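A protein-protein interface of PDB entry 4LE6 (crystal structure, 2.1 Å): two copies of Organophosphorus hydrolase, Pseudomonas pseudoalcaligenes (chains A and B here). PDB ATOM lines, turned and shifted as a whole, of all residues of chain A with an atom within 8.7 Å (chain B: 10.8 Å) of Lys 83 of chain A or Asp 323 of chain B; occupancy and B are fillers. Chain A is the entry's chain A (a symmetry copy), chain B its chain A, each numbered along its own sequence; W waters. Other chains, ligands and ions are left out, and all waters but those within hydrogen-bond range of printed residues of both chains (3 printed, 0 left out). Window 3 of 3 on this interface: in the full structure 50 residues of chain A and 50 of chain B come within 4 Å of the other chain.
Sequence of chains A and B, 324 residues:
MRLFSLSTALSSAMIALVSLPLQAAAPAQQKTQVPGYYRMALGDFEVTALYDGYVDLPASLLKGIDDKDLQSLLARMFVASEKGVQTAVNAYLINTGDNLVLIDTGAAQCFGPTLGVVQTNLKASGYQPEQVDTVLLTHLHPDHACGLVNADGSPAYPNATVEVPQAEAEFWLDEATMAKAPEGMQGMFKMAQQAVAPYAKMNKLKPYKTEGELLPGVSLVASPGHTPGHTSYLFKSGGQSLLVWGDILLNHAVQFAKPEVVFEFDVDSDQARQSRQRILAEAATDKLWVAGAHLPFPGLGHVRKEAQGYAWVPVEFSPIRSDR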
ATOM      1  N   TYR A  54       8.298  -4.097 -28.570  1.00  0.00           N
ATOM      2  CA  TYR A  54       9.368  -3.881 -27.600  1.00  0.00           C
ATOM      3  C   TYR A  54      10.277  -5.087 -27.497  1.00  0.00           C
ATOM      4  O   TYR A  54       9.915  -6.193 -27.890  1.00  0.00           O
ATOM      5  CB  TYR A  54       8.795  -3.591 -26.205  1.00  0.00           C
ATOM      6  CG  TYR A  54       7.960  -4.735 -25.649  1.00  0.00           C
ATOM      7  CD1 TYR A  54       8.540  -5.767 -24.907  1.00  0.00           C
ATOM      8  CD2 TYR A  54       6.599  -4.807 -25.892  1.00  0.00           C
ATOM      9  CE1 TYR A  54       7.784  -6.815 -24.423  1.00  0.00           C
ATOM     10  CE2 TYR A  54       5.829  -5.857 -25.386  1.00  0.00           C
ATOM     11  CZ  TYR A  54       6.432  -6.852 -24.660  1.00  0.00           C
ATOM     12  OH  TYR A  54       5.677  -7.892 -24.163  1.00  0.00           O
ATOM     13  N   VAL A  55      11.467  -4.853 -26.962  1.00  0.00           N
ATOM     14  CA  VAL A  55      12.369  -5.930 -26.605  1.00  0.00           C
ATOM     15  C   VAL A  55      12.945  -5.636 -25.202  1.00  0.00           C
ATOM     16  O   VAL A  55      13.238  -4.487 -24.873  1.00  0.00           O
ATOM     17  CB  VAL A  55      13.494  -6.066 -27.659  1.00  0.00           C
ATOM     18  CG1 VAL A  55      14.273  -4.763 -27.797  1.00  0.00           C
ATOM     19  CG2 VAL A  55      14.411  -7.211 -27.299  1.00  0.00           C
ATOM     20  N   ASP A  56      13.089  -6.660 -24.370  1.00  0.00           N
ATOM     21  CA  ASP A  56      13.688  -6.483 -23.051  1.00  0.00           C
ATOM     22  C   ASP A  56      15.213  -6.568 -23.176  1.00  0.00           C
ATOM     23  O   ASP A  56      15.740  -7.593 -23.600  1.00  0.00           O
ATOM     24  CB  ASP A  56      13.175  -7.551 -22.091  1.00  0.00           C
ATOM     25  CG  ASP A  56      11.681  -7.391 -21.755  1.00  0.00           C
ATOM     26  OD1 ASP A  56      11.124  -6.256 -21.800  1.00  0.00           O
ATOM     27  OD2 ASP A  56      11.059  -8.423 -21.430  1.00  0.00           O
ATOM     28  N   LEU A  57      15.915  -5.486 -22.842  1.00  0.00           N
ATOM     29  CA  LEU A  57      17.385  -5.455 -22.883  1.00  0.00           C
ATOM     30  C   LEU A  57      17.968  -5.405 -21.461  1.00  0.00           C
ATOM     31  O   LEU A  57      17.564  -4.558 -20.670  1.00  0.00           O
ATOM     32  CB  LEU A  57      17.860  -4.237 -23.678  1.00  0.00           C
ATOM     33  CG  LEU A  57      17.425  -4.171 -25.147  1.00  0.00           C
ATOM     34  CD1 LEU A  57      17.985  -2.902 -25.783  1.00  0.00           C
ATOM     35  CD2 LEU A  57      17.866  -5.419 -25.929  1.00  0.00           C
ATOM     36  N   PRO A  58      18.893  -6.324 -21.116  1.00  0.00           N
ATOM     37  CA  PRO A  58      19.523  -6.265 -19.786  1.00  0.00           C
ATOM     38  C   PRO A  58      20.260  -4.959 -19.574  1.00  0.00           C
ATOM     39  O   PRO A  58      20.968  -4.515 -20.476  1.00  0.00           O
ATOM     40  CB  PRO A  58      20.552  -7.409 -19.818  1.00  0.00           C
ATOM     41  CG  PRO A  58      20.064  -8.335 -20.862  1.00  0.00           C
ATOM     42  CD  PRO A  58      19.336  -7.500 -21.883  1.00  0.00           C
ATOM     43  N   ALA A  59      20.135  -4.379 -18.388  1.00  0.00           N
ATOM     44  CA  ALA A  59      20.812  -3.132 -18.080  1.00  0.00           C
ATOM     45  C   ALA A  59      22.328  -3.308 -18.155  1.00  0.00           C
ATOM     46  O   ALA A  59      23.060  -2.336 -18.327  1.00  0.00           O
ATOM     47  CB  ALA A  59      20.402  -2.651 -16.689  1.00  0.00           C
ATOM     48  N   VAL A  79      11.918   3.339 -14.314  1.00  0.00           N
ATOM     49  CA  VAL A  79      12.153   2.280 -15.295  1.00  0.00           C
ATOM     50  C   VAL A  79      12.563   1.013 -14.544  1.00  0.00           C
ATOM     51  O   VAL A  79      13.567   1.004 -13.831  1.00  0.00           O
ATOM     52  CB  VAL A  79      13.257   2.671 -16.307  1.00  0.00           C
ATOM     53  CG1 VAL A  79      13.463   1.573 -17.357  1.00  0.00           C
ATOM     54  CG2 VAL A  79      12.907   3.982 -16.996  1.00  0.00           C
ATOM     55  N   ALA A  80      11.780  -0.050 -14.698  1.00  0.00           N
ATOM     56  CA  ALA A  80      12.083  -1.328 -14.067  1.00  0.00           C
ATOM     57  C   ALA A  80      13.179  -2.015 -14.864  1.00  0.00           C
ATOM     58  O   ALA A  80      13.234  -1.870 -16.088  1.00  0.00           O
ATOM     59  CB  ALA A  80      10.830  -2.198 -14.037  1.00  0.00           C
ATOM     60  N   SER A  81      14.051  -2.758 -14.185  1.00  0.00           N
ATOM     61  CA  SER A  81      15.203  -3.385 -14.843  1.00  0.00           C
ATOM     62  C   SER A  81      15.431  -4.833 -14.391  1.00  0.00           C
ATOM     63  O   SER A  81      16.331  -5.508 -14.899  1.00  0.00           O
ATOM     64  CB  SER A  81      16.470  -2.567 -14.565  1.00  0.00           C
ATOM     65  OG  SER A  81      16.639  -2.368 -13.169  1.00  0.00           O
ATOM     66  N   GLU A  82      14.623  -5.310 -13.449  1.00  0.00           N
ATOM     67  CA  GLU A  82      14.837  -6.636 -12.856  1.00  0.00           C
ATOM     68  C   GLU A  82      14.740  -7.756 -13.895  1.00  0.00           C
ATOM     69  O   GLU A  82      15.416  -8.771 -13.783  1.00  0.00           O
ATOM     70  CB  GLU A  82      13.845  -6.889 -11.715  1.00  0.00           C
ATOM     71  CG  GLU A  82      14.095  -6.050 -10.476  1.00  0.00           C
ATOM     72  CD  GLU A  82      12.987  -6.178  -9.446  1.00  0.00           C
ATOM     73  OE1 GLU A  82      11.994  -6.884  -9.720  1.00  0.00           O
ATOM     74  OE2 GLU A  82      13.108  -5.571  -8.361  1.00  0.00           O
ATOM     75  N   LYS A  83      13.905  -7.555 -14.908  1.00  0.00           N
ATOM     76  CA  LYS A  83      13.745  -8.526 -15.982  1.00  0.00           C
ATOM     77  C   LYS A  83      14.203  -7.909 -17.304  1.00  0.00           C
ATOM     78  O   LYS A  83      13.818  -8.355 -18.381  1.00  0.00           O
ATOM     79  CB  LYS A  83      12.286  -8.996 -16.047  1.00  0.00           C
ATOM     80  CG  LYS A  83      11.972 -10.132 -15.061  1.00  0.00           C
ATOM     81  CD  LYS A  83      10.511 -10.132 -14.635  1.00  0.00           C
ATOM     82  CE  LYS A  83      10.040 -11.515 -14.214  1.00  0.00           C
ATOM     83  NZ  LYS A  83       8.556 -11.610 -14.260  1.00  0.00           N
ATOM     84  N   GLY A  84      15.059  -6.896 -17.203  1.00  0.00           N
ATOM     85  CA  GLY A  84      15.554  -6.189 -18.367  1.00  0.00           C
ATOM     86  C   GLY A  84      14.779  -4.911 -18.597  1.00  0.00           C
ATOM     87  O   GLY A  84      13.655  -4.770 -18.118  1.00  0.00           O
ATOM     88  N   VAL A  85      15.378  -3.982 -19.336  1.00  0.00           N
ATOM     89  CA  VAL A  85      14.744  -2.712 -19.651  1.00  0.00           C
ATOM     90  C   VAL A  85      13.875  -2.872 -20.892  1.00  0.00           C
ATOM     91  O   VAL A  85      14.363  -3.139 -21.989  1.00  0.00           O
ATOM     92  CB  VAL A  85      15.796  -1.618 -19.897  1.00  0.00           C
ATOM     93  CG1 VAL A  85      15.143  -0.314 -20.366  1.00  0.00           C
ATOM     94  CG2 VAL A  85      16.619  -1.399 -18.637  1.00  0.00           C
ATOM     95  N   GLN A  86      12.572  -2.738 -20.717  1.00  0.00           N
ATOM     96  CA  GLN A  86      11.665  -2.843 -21.849  1.00  0.00           C
ATOM     97  C   GLN A  86      11.917  -1.680 -22.784  1.00  0.00           C
ATOM     98  O   GLN A  86      11.695  -0.527 -22.415  1.00  0.00           O
ATOM     99  CB  GLN A  86      10.218  -2.816 -21.382  1.00  0.00           C
ATOM    100  CG  GLN A  86       9.208  -2.854 -22.531  1.00  0.00           C
ATOM    101  CD  GLN A  86       7.789  -2.963 -22.010  1.00  0.00           C
ATOM    102  OE1 GLN A  86       7.575  -3.301 -20.849  1.00  0.00           O
ATOM    103  NE2 GLN A  86       6.826  -2.646 -22.840  1.00  0.00           N
ATOM    104  N   THR A  87      12.362  -1.992 -23.994  1.00  0.00           N
ATOM    105  CA  THR A  87      12.824  -0.987 -24.912  1.00  0.00           C
ATOM    106  C   THR A  87      11.948  -0.994 -26.166  1.00  0.00           C
ATOM    107  O   THR A  87      11.721  -2.034 -26.780  1.00  0.00           O
ATOM    108  CB  THR A  87      14.288  -1.229 -25.277  1.00  0.00           C
ATOM    109  OG1 THR A  87      15.092  -1.172 -24.092  1.00  0.00           O
ATOM    110  CG2 THR A  87      14.785  -0.185 -26.267  1.00  0.00           C
ATOM    111  N   THR A 114       7.113 -10.162 -29.783  1.00  0.00           N
ATOM    112  CA  THR A 114       6.849  -8.859 -29.146  1.00  0.00           C
ATOM    113  C   THR A 114       7.211  -7.699 -30.081  1.00  0.00           C
ATOM    114  O   THR A 114       7.028  -6.533 -29.740  1.00  0.00           O
ATOM    115  CB  THR A 114       7.613  -8.696 -27.799  1.00  0.00           C
ATOM    116  OG1 THR A 114       9.024  -8.645 -28.037  1.00  0.00           O
ATOM    117  CG2 THR A 114       7.271  -9.830 -26.876  1.00  0.00           C
ATOM    118  N   ALA B  41      -2.477  -1.535 -17.185  1.00  0.00           N
ATOM    119  CA  ALA B  41      -2.854  -2.452 -16.124  1.00  0.00           C
ATOM    120  C   ALA B  41      -2.531  -1.808 -14.784  1.00  0.00           C
ATOM    121  O   ALA B  41      -1.538  -1.109 -14.641  1.00  0.00           O
ATOM    122  CB  ALA B  41      -2.116  -3.770 -16.267  1.00  0.00           C
ATOM    123  N   SER B 318       3.237   1.214 -23.785  1.00  0.00           N
ATOM    124  CA  SER B 318       3.452  -0.224 -23.696  1.00  0.00           C
ATOM    125  C   SER B 318       2.152  -0.970 -23.895  1.00  0.00           C
ATOM    126  O   SER B 318       1.105  -0.536 -23.426  1.00  0.00           O
ATOM    127  CB  SER B 318       3.992  -0.600 -22.313  1.00  0.00           C
ATOM    128  OG  SER B 318       4.125  -2.008 -22.182  1.00  0.00           O
ATOM    129  N   PRO B 319       2.210  -2.120 -24.565  1.00  0.00           N
ATOM    130  CA  PRO B 319       1.028  -2.975 -24.435  1.00  0.00           C
ATOM    131  C   PRO B 319       0.893  -3.490 -23.011  1.00  0.00           C
ATOM    132  O   PRO B 319       1.827  -3.409 -22.206  1.00  0.00           O
ATOM    133  CB  PRO B 319       1.307  -4.133 -25.400  1.00  0.00           C
ATOM    134  CG  PRO B 319       2.776  -4.088 -25.684  1.00  0.00           C
ATOM    135  CD  PRO B 319       3.232  -2.681 -25.460  1.00  0.00           C
ATOM    136  N   ILE B 320      -0.272  -4.040 -22.699  1.00  0.00           N
ATOM    137  CA  ILE B 320      -0.440  -4.760 -21.456  1.00  0.00           C
ATOM    138  C   ILE B 320       0.237  -6.114 -21.615  1.00  0.00           C
ATOM    139  O   ILE B 320      -0.042  -6.864 -22.549  1.00  0.00           O
ATOM    140  CB  ILE B 320      -1.933  -4.866 -21.104  1.00  0.00           C
ATOM    141  CG1 ILE B 320      -2.411  -3.472 -20.662  1.00  0.00           C
ATOM    142  CG2 ILE B 320      -2.188  -5.922 -20.011  1.00  0.00           C
ATOM    143  CD1 ILE B 320      -3.891  -3.350 -20.468  1.00  0.00           C
ATOM    144  N   ARG B 321       1.156  -6.401 -20.713  1.00  0.00           N
ATOM    145  CA  ARG B 321       1.996  -7.580 -20.824  1.00  0.00           C
ATOM    146  C   ARG B 321       1.461  -8.702 -19.953  1.00  0.00           C
ATOM    147  O   ARG B 321       1.114  -8.478 -18.802  1.00  0.00           O
ATOM    148  CB  ARG B 321       3.421  -7.230 -20.415  1.00  0.00           C
ATOM    149  CG  ARG B 321       4.081  -6.273 -21.374  1.00  0.00           C
ATOM    150  CD  ARG B 321       5.540  -6.044 -21.024  1.00  0.00           C
ATOM    151  NE  ARG B 321       6.337  -7.275 -21.055  1.00  0.00           N
ATOM    152  CZ  ARG B 321       7.667  -7.293 -21.065  1.00  0.00           C
ATOM    153  NH1 ARG B 321       8.328  -8.440 -21.090  1.00  0.00           N
ATOM    154  NH2 ARG B 321       8.342  -6.154 -21.048  1.00  0.00           N
ATOM    155  N   SER B 322       1.391  -9.897 -20.530  1.00  0.00           N
ATOM    156  CA  SER B 322       0.952 -11.098 -19.827  1.00  0.00           C
ATOM    157  C   SER B 322       2.021 -11.556 -18.850  1.00  0.00           C
ATOM    158  O   SER B 322       1.717 -12.145 -17.818  1.00  0.00           O
ATOM    159  CB  SER B 322       0.709 -12.223 -20.836  1.00  0.00           C
ATOM    160  OG  SER B 322      -0.080 -11.777 -21.926  1.00  0.00           O
ATOM    161  N   ASP B 323       3.280 -11.291 -19.195  1.00  0.00           N
ATOM    162  CA  ASP B 323       4.408 -11.769 -18.407  1.00  0.00           C
ATOM    163  C   ASP B 323       4.826 -10.745 -17.349  1.00  0.00           C
ATOM    164  O   ASP B 323       5.979 -10.721 -16.921  1.00  0.00           O
ATOM    165  CB  ASP B 323       5.588 -12.136 -19.324  1.00  0.00           C
ATOM    166  CG  ASP B 323       6.051 -10.974 -20.204  1.00  0.00           C
ATOM    167  OD1 ASP B 323       5.284 -10.015 -20.418  1.00  0.00           O
ATOM    168  OD2 ASP B 323       7.197 -11.029 -20.694  1.00  0.00           O
ATOM    169  N   ARG B 324       3.882  -9.902 -16.938  1.00  0.00           N
ATOM    170  CA  ARG B 324       4.127  -8.903 -15.893  1.00  0.00           C
ATOM    171  C   ARG B 324       2.940  -8.807 -14.942  1.00  0.00           C
ATOM    172  O   ARG B 324       1.816  -9.138 -15.311  1.00  0.00           O
ATOM    173  CB  ARG B 324       4.398  -7.524 -16.499  1.00  0.00           C
ATOM    174  CG  ARG B 324       5.623  -7.461 -17.400  1.00  0.00           C
ATOM    175  CD  ARG B 324       6.906  -7.705 -16.624  1.00  0.00           C
ATOM    176  NE  ARG B 324       7.673  -8.814 -17.194  1.00  0.00           N
ATOM    177  CZ  ARG B 324       8.842  -8.698 -17.820  1.00  0.00           C
ATOM    178  NH1 ARG B 324       9.423  -7.513 -17.970  1.00  0.00           N
ATOM    179  NH2 ARG B 324       9.440  -9.785 -18.294  1.00  0.00           N
HETATM  180  O   HOH W   1       6.578 -10.445 -23.425  1.00  0.00           O
HETATM  181  O   HOH W   2      11.019  -5.768 -18.780  1.00  0.00           O
HETATM  182  O   HOH W   3       5.354  -2.169 -19.429  1.00  0.00           O
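Asp 56 of chain A touches just these residues of chain B: Arg 321 and Arg 324. Ala 59 of chain A touches none of the printed residues of chain B. Lys 83 of chain A touches just these residues of chain B: Asp 323 and Arg 324. No residue of chain B comes within 4 Å of Gly 84 of chain A. Of the printed residues of chain B, Gln 86 of chain A touches Ser 318 and Arg 321. Of the printed residues of chain A, Pro 319 of chain B touches Tyr 54 (3.5 Å). No residue of chain A comes within 4 Å of Ser 322 of chain B. Arg 324 of chain B touches two residues of chain A. The nearest printed residue of chain A that does not touch Ser 318 of chain B is Tyr 54 of chain A (5.3 Å).
The side-chain carboxylate (OD2) of Asp 323 of chain B lies within salt-bridge range of the guanidinium group (NH1) of Arg 321 of chain B (2.9 Å). OD2 of Asp 323 of chain B lies within salt-bridge range of NH2 of Arg 324 of chain B. OG1 of Thr 114 of chain A is in hydrogen-bond range of O of Tyr 54 of chain A (2.6 Å).
No position is printed for both chains. Of the 8 pairs that touch across the chains among the printed residues, none has its exchanged pair printed and touching as well.
Of the 8 printed residues of chain B, 5 touch a printed residue of chain A. Printed residues of chain B that touch a printed residue of chain A: Ser 318, Pro 319, Arg 321, Asp 323 and Arg 324. Hydrophobic or aromatic side chains of chain B that line the printed part of chain A: Pro 319. Printed residues of chain A that touch a printed residue of chain B: Tyr 54, Asp 56, Lys 83 and Gln 86.
Water W2 lies within hydrogen-bond range of NH1 of Arg 324 of chain B (2.5 Å), O of Gly 84 of chain A (2.9 Å) and OD1 of Asp 56 of chain A (3.1 Å). Water W1 bridges the side-chain hydroxyl (OH) of Tyr 54 of chain A and the side-chain carboxylate (OD2) of Asp 323 of chain B. Water W3 lies within hydrogen-bond range of OE1 of Gln 86 of chain A (2.9 Å) and OG of Ser 318 of chain B (3.0 Å).
Pro 319 of chain B touches Tyr 54 of chain A. NZ of Lys 83 of chain A touches O of Asp 323 of chain B, 3.8 Å away. Lys 83 of chain A touches Arg 324 of chain B (CB to NH2, 3.7 Å).
OG of Ser 318 of chain B sits at hydrogen-bond distance from NE2 of Gln 86 of chain A (2.9 Å). NE of Arg 321 of chain B sits at hydrogen-bond distance from OH of Tyr 54 of chain A (3.2 Å). The side-chain carboxylate (OD2) of Asp 56 of chain A lies within salt-bridge range of the guanidinium group (NH1) of Arg 321 of chain B, at 2.8 Å. NH2 of Arg 321 of chain B lies within hydrogen-bond range of OE1 of Gln 86 of chain A, at 3.0 Å. NH2 of Arg 324 of chain B lies within salt-bridge range of OD2 of Asp 56 of chain A (3.8 Å).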
